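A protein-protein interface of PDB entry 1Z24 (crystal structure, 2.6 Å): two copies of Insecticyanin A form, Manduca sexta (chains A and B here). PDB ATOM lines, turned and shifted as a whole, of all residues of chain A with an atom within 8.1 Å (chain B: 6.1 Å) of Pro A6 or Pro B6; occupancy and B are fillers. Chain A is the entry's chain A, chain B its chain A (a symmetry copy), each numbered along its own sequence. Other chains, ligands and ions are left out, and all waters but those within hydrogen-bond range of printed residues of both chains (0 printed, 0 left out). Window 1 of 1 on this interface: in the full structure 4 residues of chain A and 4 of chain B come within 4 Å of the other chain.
Tyr A5 touches Pro B6, and with the chains exchanged Pro A6 touches Tyr B5.
Pro A6 touches its own counterpart, Pro B6.
Of the 3 pairs that touch across the chains among the printed residues, 3 have their exchanged pair printed and touching as well.
Among the printed residues, pairs that only touch across the chains: Pro A6 with Tyr B5 (3.7 Å), Tyr A5 with Pro B6 (3.7 Å) and Pro A6 with Pro B6 (3.8 Å).
Of the 16 printed residues of chain A, 2 touch a printed residue of chain B.
Hydrophobic or aromatic side chains of chain A that line the printed part of chain B: Tyr A5 and Pro A6.
Along chain A the printed residues that touch a printed residue of chain B span positions 5 to 6.
Among the printed residues, 3 pairs touch across the chains.
Among the printed residues, no Asp or Glu carboxylate lies within 4 Å of a Lys or Arg side-chain nitrogen of the other chain.
Printed residues of chain B within 4 Å of Pro A6: Tyr B5 and Pro B6.
Of the printed residues of chain A, Pro B6 touches Tyr A5 (3.7 Å) and Pro A6 (3.8 Å).
Gly B7 touches none of the printed residues of chain A.
Of the printed residues of chain B, Tyr A5 touches Pro B6 (3.7 Å).
Printed residues of chain A within 4 Å of Tyr B5: Pro A6 (3.7 Å).
His B128 touches none of the printed residues of chain A.
N of Tyr A5 sits at hydrogen-bond distance from O of His A128.
The backbone NH (N) of Tyr B5 sits at hydrogen-bond distance from the backbone carbonyl oxygen (O) of His B128, 2.7 Å away.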
ATOM      1  N   ILE A   3      -3.375 -11.525  24.126  1.00  0.00           N
ATOM      2  CA  ILE A   3      -2.825 -12.812  24.524  1.00  0.00           C
ATOM      3  C   ILE A   3      -3.643 -14.010  23.989  1.00  0.00           C
ATOM      4  O   ILE A   3      -4.840 -14.148  24.228  1.00  0.00           O
ATOM      5  CB  ILE A   3      -2.592 -12.913  26.040  1.00  0.00           C
ATOM      6  CG1 ILE A   3      -1.619 -11.857  26.498  1.00  0.00           C
ATOM      7  CG2 ILE A   3      -2.062 -14.285  26.463  1.00  0.00           C
ATOM      8  CD1 ILE A   3      -2.119 -11.249  27.771  1.00  0.00           C
ATOM      9  N   PHE A   4      -2.992 -14.899  23.252  1.00  0.00           N
ATOM     10  CA  PHE A   4      -3.655 -16.078  22.713  1.00  0.00           C
ATOM     11  C   PHE A   4      -3.020 -17.320  23.258  1.00  0.00           C
ATOM     12  O   PHE A   4      -1.846 -17.372  23.581  1.00  0.00           O
ATOM     13  CB  PHE A   4      -3.357 -16.098  21.187  1.00  0.00           C
ATOM     14  CG  PHE A   4      -4.358 -15.352  20.362  1.00  0.00           C
ATOM     15  CD1 PHE A   4      -4.205 -13.979  20.173  1.00  0.00           C
ATOM     16  CD2 PHE A   4      -5.445 -16.037  19.814  1.00  0.00           C
ATOM     17  CE1 PHE A   4      -5.143 -13.291  19.402  1.00  0.00           C
ATOM     18  CE2 PHE A   4      -6.383 -15.369  19.050  1.00  0.00           C
ATOM     19  CZ  PHE A   4      -6.203 -14.004  18.838  1.00  0.00           C
ATOM     20  N   TYR A   5      -3.794 -18.326  23.363  1.00  0.00           N
ATOM     21  CA  TYR A   5      -3.300 -19.593  23.833  1.00  0.00           C
ATOM     22  C   TYR A   5      -3.930 -20.605  22.902  1.00  0.00           C
ATOM     23  O   TYR A   5      -4.985 -20.342  22.324  1.00  0.00           O
ATOM     24  CB  TYR A   5      -3.834 -19.880  25.178  1.00  0.00           C
ATOM     25  CG  TYR A   5      -3.372 -18.937  26.208  1.00  0.00           C
ATOM     26  CD1 TYR A   5      -2.126 -19.139  26.804  1.00  0.00           C
ATOM     27  CD2 TYR A   5      -4.151 -17.858  26.632  1.00  0.00           C
ATOM     28  CE1 TYR A   5      -1.654 -18.299  27.824  1.00  0.00           C
ATOM     29  CE2 TYR A   5      -3.703 -17.028  27.672  1.00  0.00           C
ATOM     30  CZ  TYR A   5      -2.462 -17.262  28.282  1.00  0.00           C
ATOM     31  OH  TYR A   5      -1.969 -16.476  29.290  1.00  0.00           O
ATOM     32  N   PRO A   6      -3.321 -21.743  22.725  1.00  0.00           N
ATOM     33  CA  PRO A   6      -3.876 -22.716  21.817  1.00  0.00           C
ATOM     34  C   PRO A   6      -5.118 -23.423  22.250  1.00  0.00           C
ATOM     35  O   PRO A   6      -5.356 -23.601  23.423  1.00  0.00           O
ATOM     36  CB  PRO A   6      -2.830 -23.788  21.604  1.00  0.00           C
ATOM     37  CG  PRO A   6      -1.773 -23.566  22.668  1.00  0.00           C
ATOM     38  CD  PRO A   6      -2.007 -22.158  23.243  1.00  0.00           C
ATOM     39  N   GLY A   7      -5.917 -23.841  21.283  1.00  0.00           N
ATOM     40  CA  GLY A   7      -7.118 -24.584  21.611  1.00  0.00           C
ATOM     41  C   GLY A   7      -8.340 -23.770  21.892  1.00  0.00           C
ATOM     42  O   GLY A   7      -8.335 -22.554  21.736  1.00  0.00           O
ATOM     43  N   TYR A   8      -9.384 -24.496  22.305  1.00  0.00           N
ATOM     44  CA  TYR A   8     -10.674 -23.887  22.619  1.00  0.00           C
ATOM     45  C   TYR A   8     -10.601 -23.224  23.966  1.00  0.00           C
ATOM     46  O   TYR A   8      -9.717 -23.542  24.738  1.00  0.00           O
ATOM     47  CB  TYR A   8     -11.775 -25.043  22.710  1.00  0.00           C
ATOM     48  CG  TYR A   8     -12.011 -25.769  21.402  1.00  0.00           C
ATOM     49  CD1 TYR A   8     -12.687 -25.168  20.356  1.00  0.00           C
ATOM     50  CD2 TYR A   8     -11.526 -27.046  21.168  1.00  0.00           C
ATOM     51  CE1 TYR A   8     -12.929 -25.814  19.138  1.00  0.00           C
ATOM     52  CE2 TYR A   8     -11.723 -27.703  19.961  1.00  0.00           C
ATOM     53  CZ  TYR A   8     -12.425 -27.088  18.927  1.00  0.00           C
ATOM     54  OH  TYR A   8     -12.615 -27.732  17.708  1.00  0.00           O
ATOM     55  N   CYS A   9     -11.539 -22.331  24.256  1.00  0.00           N
ATOM     56  CA  CYS A   9     -11.537 -21.670  25.552  1.00  0.00           C
ATOM     57  C   CYS A   9     -11.746 -22.717  26.586  1.00  0.00           C
ATOM     58  O   CYS A   9     -12.455 -23.641  26.274  1.00  0.00           O
ATOM     59  CB  CYS A   9     -12.850 -20.832  25.550  1.00  0.00           C
ATOM     60  SG  CYS A   9     -12.601 -19.393  24.527  1.00  0.00           S
ATOM     61  N   PRO A  10     -11.171 -22.600  27.785  1.00  0.00           N
ATOM     62  CA  PRO A  10     -11.359 -23.607  28.819  1.00  0.00           C
ATOM     63  C   PRO A  10     -12.693 -23.494  29.507  1.00  0.00           C
ATOM     64  O   PRO A  10     -13.435 -22.491  29.405  1.00  0.00           O
ATOM     65  CB  PRO A  10     -10.427 -23.277  29.971  1.00  0.00           C
ATOM     66  CG  PRO A  10     -10.066 -21.836  29.708  1.00  0.00           C
ATOM     67  CD  PRO A  10     -10.081 -21.724  28.193  1.00  0.00           C
ATOM     68  N   TYR A 121     -12.716 -17.382  20.983  1.00  0.00           N
ATOM     69  CA  TYR A 121     -12.135 -18.451  20.168  1.00  0.00           C
ATOM     70  C   TYR A 121     -12.053 -18.119  18.675  1.00  0.00           C
ATOM     71  O   TYR A 121     -13.039 -17.719  18.097  1.00  0.00           O
ATOM     72  CB  TYR A 121     -12.802 -19.845  20.460  1.00  0.00           C
ATOM     73  CG  TYR A 121     -12.195 -20.974  19.600  1.00  0.00           C
ATOM     74  CD1 TYR A 121     -10.940 -21.519  19.862  1.00  0.00           C
ATOM     75  CD2 TYR A 121     -12.866 -21.503  18.495  1.00  0.00           C
ATOM     76  CE1 TYR A 121     -10.374 -22.506  19.061  1.00  0.00           C
ATOM     77  CE2 TYR A 121     -12.360 -22.537  17.704  1.00  0.00           C
ATOM     78  CZ  TYR A 121     -11.087 -23.009  17.979  1.00  0.00           C
ATOM     79  OH  TYR A 121     -10.561 -23.949  17.202  1.00  0.00           O
ATOM     80  N   LYS A 125      -7.659 -19.993  13.806  1.00  0.00           N
ATOM     81  CA  LYS A 125      -6.313 -20.051  14.319  1.00  0.00           C
ATOM     82  C   LYS A 125      -6.187 -21.188  15.276  1.00  0.00           C
ATOM     83  O   LYS A 125      -5.089 -21.453  15.708  1.00  0.00           O
ATOM     84  CB  LYS A 125      -5.906 -18.846  15.147  1.00  0.00           C
ATOM     85  CG  LYS A 125      -5.734 -17.614  14.255  1.00  0.00           C
ATOM     86  CD  LYS A 125      -5.510 -16.295  14.994  1.00  0.00           C
ATOM     87  CE  LYS A 125      -4.543 -16.433  16.175  1.00  0.00           C
ATOM     88  NZ  LYS A 125      -3.451 -15.434  16.262  1.00  0.00           N
ATOM     89  N   LYS A 126      -7.319 -21.837  15.593  1.00  0.00           N
ATOM     90  CA  LYS A 126      -7.329 -22.912  16.553  1.00  0.00           C
ATOM     91  C   LYS A 126      -6.689 -22.403  17.835  1.00  0.00           C
ATOM     92  O   LYS A 126      -5.908 -23.066  18.464  1.00  0.00           O
ATOM     93  CB  LYS A 126      -6.736 -24.238  16.143  1.00  0.00           C
ATOM     94  CG  LYS A 126      -7.317 -24.730  14.809  1.00  0.00           C
ATOM     95  CD  LYS A 126      -8.044 -26.055  15.001  1.00  0.00           C
ATOM     96  CE  LYS A 126      -8.210 -26.864  13.719  1.00  0.00           C
ATOM     97  NZ  LYS A 126      -9.535 -26.692  13.091  1.00  0.00           N
ATOM     98  N   ALA A 127      -7.010 -21.195  18.226  1.00  0.00           N
ATOM     99  CA  ALA A 127      -6.464 -20.630  19.448  1.00  0.00           C
ATOM    100  C   ALA A 127      -7.461 -19.613  19.983  1.00  0.00           C
ATOM    101  O   ALA A 127      -8.383 -19.168  19.273  1.00  0.00           O
ATOM    102  CB  ALA A 127      -5.127 -19.978  19.173  1.00  0.00           C
ATOM    103  N   HIS A 128      -7.299 -19.231  21.242  1.00  0.00           N
ATOM    104  CA  HIS A 128      -8.219 -18.259  21.791  1.00  0.00           C
ATOM    105  C   HIS A 128      -7.432 -17.182  22.462  1.00  0.00           C
ATOM    106  O   HIS A 128      -6.288 -17.375  22.936  1.00  0.00           O
ATOM    107  CB  HIS A 128      -9.253 -18.887  22.855  1.00  0.00           C
ATOM    108  CG  HIS A 128      -8.505 -19.648  23.911  1.00  0.00           C
ATOM    109  ND1 HIS A 128      -7.937 -20.904  23.647  1.00  0.00           N
ATOM    110  CD2 HIS A 128      -8.223 -19.321  25.195  1.00  0.00           C
ATOM    111  CE1 HIS A 128      -7.336 -21.278  24.770  1.00  0.00           C
ATOM    112  NE2 HIS A 128      -7.480 -20.369  25.728  1.00  0.00           N
ATOM    113  N   SER A 129      -8.066 -16.022  22.494  1.00  0.00           N
ATOM    114  CA  SER A 129      -7.436 -14.915  23.179  1.00  0.00           C
ATOM    115  C   SER A 129      -8.145 -14.785  24.539  1.00  0.00           C
ATOM    116  O   SER A 129      -9.321 -15.134  24.672  1.00  0.00           O
ATOM    117  CB  SER A 129      -7.449 -13.564  22.486  1.00  0.00           C
ATOM    118  OG  SER A 129      -8.756 -13.238  22.016  1.00  0.00           O
ATOM    119  N   HIS A 158      -5.208 -20.767  36.817  1.00  0.00           N
ATOM    120  CA  HIS A 158      -5.223 -21.611  35.610  1.00  0.00           C
ATOM    121  C   HIS A 158      -6.014 -20.984  34.491  1.00  0.00           C
ATOM    122  O   HIS A 158      -6.177 -21.566  33.434  1.00  0.00           O
ATOM    123  CB  HIS A 158      -5.878 -22.988  35.911  1.00  0.00           C
ATOM    124  CG  HIS A 158      -7.286 -22.894  36.384  1.00  0.00           C
ATOM    125  ND1 HIS A 158      -7.629 -22.263  37.556  1.00  0.00           N
ATOM    126  CD2 HIS A 158      -8.433 -23.374  35.818  1.00  0.00           C
ATOM    127  CE1 HIS A 158      -8.930 -22.352  37.679  1.00  0.00           C
ATOM    128  NE2 HIS A 158      -9.444 -23.023  36.651  1.00  0.00           N
ATOM    129  N   ASP A 161      -3.233 -15.365  33.728  1.00  0.00           N
ATOM    130  CA  ASP A 161      -1.876 -15.223  34.121  1.00  0.00           C
ATOM    131  C   ASP A 161      -1.753 -13.778  34.650  1.00  0.00           C
ATOM    132  O   ASP A 161      -1.631 -12.789  33.902  1.00  0.00           O
ATOM    133  CB  ASP A 161      -1.039 -15.425  32.904  1.00  0.00           C
ATOM    134  CG  ASP A 161       0.463 -15.179  33.176  1.00  0.00           C
ATOM    135  OD1 ASP A 161       1.277 -15.434  32.354  1.00  0.00           O
ATOM    136  OD2 ASP A 161       0.845 -14.749  34.357  1.00  0.00           O
ATOM    137  N   PHE B   4       3.366 -29.841  24.440  1.00  0.00           N
ATOM    138  CA  PHE B   4       3.232 -28.954  25.587  1.00  0.00           C
ATOM    139  C   PHE B   4       2.324 -27.811  25.248  1.00  0.00           C
ATOM    140  O   PHE B   4       2.212 -27.371  24.118  1.00  0.00           O
ATOM    141  CB  PHE B   4       4.629 -28.314  25.822  1.00  0.00           C
ATOM    142  CG  PHE B   4       5.512 -29.103  26.737  1.00  0.00           C
ATOM    143  CD1 PHE B   4       6.292 -30.136  26.217  1.00  0.00           C
ATOM    144  CD2 PHE B   4       5.524 -28.811  28.103  1.00  0.00           C
ATOM    145  CE1 PHE B   4       7.112 -30.867  27.077  1.00  0.00           C
ATOM    146  CE2 PHE B   4       6.330 -29.527  28.967  1.00  0.00           C
ATOM    147  CZ  PHE B   4       7.131 -30.534  28.432  1.00  0.00           C
ATOM    148  N   TYR B   5       1.672 -27.325  26.229  1.00  0.00           N
ATOM    149  CA  TYR B   5       0.797 -26.198  26.049  1.00  0.00           C
ATOM    150  C   TYR B   5       1.087 -25.310  27.239  1.00  0.00           C
ATOM    151  O   TYR B   5       1.536 -25.794  28.278  1.00  0.00           O
ATOM    152  CB  TYR B   5      -0.611 -26.620  26.181  1.00  0.00           C
ATOM    153  CG  TYR B   5      -1.047 -27.553  25.131  1.00  0.00           C
ATOM    154  CD1 TYR B   5      -1.453 -27.044  23.896  1.00  0.00           C
ATOM    155  CD2 TYR B   5      -1.094 -28.933  25.336  1.00  0.00           C
ATOM    156  CE1 TYR B   5      -1.922 -27.883  22.874  1.00  0.00           C
ATOM    157  CE2 TYR B   5      -1.589 -29.780  24.332  1.00  0.00           C
ATOM    158  CZ  TYR B   5      -2.023 -29.252  23.107  1.00  0.00           C
ATOM    159  OH  TYR B   5      -2.501 -30.032  22.088  1.00  0.00           O
ATOM    160  N   PRO B   6       0.861 -24.031  27.124  1.00  0.00           N
ATOM    161  CA  PRO B   6       1.160 -23.152  28.227  1.00  0.00           C
ATOM    162  C   PRO B   6       0.265 -23.225  29.420  1.00  0.00           C
ATOM    163  O   PRO B   6      -0.893 -23.557  29.309  1.00  0.00           O
ATOM    164  CB  PRO B   6       1.068 -21.732  27.713  1.00  0.00           C
ATOM    165  CG  PRO B   6       0.395 -21.814  26.357  1.00  0.00           C
ATOM    166  CD  PRO B   6       0.445 -23.290  25.923  1.00  0.00           C
ATOM    167  N   GLY B   7       0.812 -22.899  30.578  1.00  0.00           N
ATOM    168  CA  GLY B   7       0.001 -22.891  31.781  1.00  0.00           C
ATOM    169  C   GLY B   7      -0.106 -24.190  32.511  1.00  0.00           C
ATOM    170  O   GLY B   7       0.551 -25.164  32.164  1.00  0.00           O
ATOM    171  N   TYR B   8      -0.958 -24.156  33.542  1.00  0.00           N
ATOM    172  CA  TYR B   8      -1.195 -25.322  34.389  1.00  0.00           C
ATOM    173  C   TYR B   8      -2.097 -26.288  33.673  1.00  0.00           C
ATOM    174  O   TYR B   8      -2.770 -25.893  32.740  1.00  0.00           O
ATOM    175  CB  TYR B   8      -1.954 -24.846  35.713  1.00  0.00           C
ATOM    176  CG  TYR B   8      -1.141 -23.908  36.582  1.00  0.00           C
ATOM    177  CD1 TYR B   8      -0.069 -24.365  37.326  1.00  0.00           C
ATOM    178  CD2 TYR B   8      -1.395 -22.547  36.640  1.00  0.00           C
ATOM    179  CE1 TYR B   8       0.698 -23.528  38.145  1.00  0.00           C
ATOM    180  CE2 TYR B   8      -0.636 -21.685  37.420  1.00  0.00           C
ATOM    181  CZ  TYR B   8       0.427 -22.168  38.179  1.00  0.00           C
ATOM    182  OH  TYR B   8       1.204 -21.310  38.951  1.00  0.00           O
ATOM    183  N   LYS B 126       6.487 -23.343  33.016  1.00  0.00           N
ATOM    184  CA  LYS B 126       5.175 -22.751  33.063  1.00  0.00           C
ATOM    185  C   LYS B 126       4.360 -23.324  31.914  1.00  0.00           C
ATOM    186  O   LYS B 126       3.650 -22.635  31.231  1.00  0.00           O
ATOM    187  CB  LYS B 126       5.073 -21.246  33.099  1.00  0.00           C
ATOM    188  CG  LYS B 126       5.951 -20.645  34.207  1.00  0.00           C
ATOM    189  CD  LYS B 126       5.094 -19.899  35.221  1.00  0.00           C
ATOM    190  CE  LYS B 126       5.860 -18.871  36.046  1.00  0.00           C
ATOM    191  NZ  LYS B 126       6.269 -19.377  37.371  1.00  0.00           N
ATOM    192  N   ALA B 127       4.474 -24.608  31.681  1.00  0.00           N
ATOM    193  CA  ALA B 127       3.720 -25.248  30.617  1.00  0.00           C
ATOM    194  C   ALA B 127       3.510 -26.706  31.000  1.00  0.00           C
ATOM    195  O   ALA B 127       4.176 -27.244  31.905  1.00  0.00           O
ATOM    196  CB  ALA B 127       4.467 -25.139  29.306  1.00  0.00           C
ATOM    197  N   HIS B 128       2.582 -27.368  30.324  1.00  0.00           N
ATOM    198  CA  HIS B 128       2.353 -28.759  30.649  1.00  0.00           C
ATOM    199  C   HIS B 128       2.349 -29.551  29.382  1.00  0.00           C
ATOM    200  O   HIS B 128       2.037 -29.053  28.276  1.00  0.00           O
ATOM    201  CB  HIS B 128       0.966 -29.014  31.427  1.00  0.00           C
ATOM    202  CG  HIS B 128      -0.171 -28.396  30.668  1.00  0.00           C
ATOM    203  ND1 HIS B 128      -0.377 -27.008  30.655  1.00  0.00           N
ATOM    204  CD2 HIS B 128      -1.125 -28.968  29.895  1.00  0.00           C
ATOM    205  CE1 HIS B 128      -1.433 -26.800  29.880  1.00  0.00           C
ATOM    206  NE2 HIS B 128      -1.921 -27.940  29.402  1.00  0.00           N
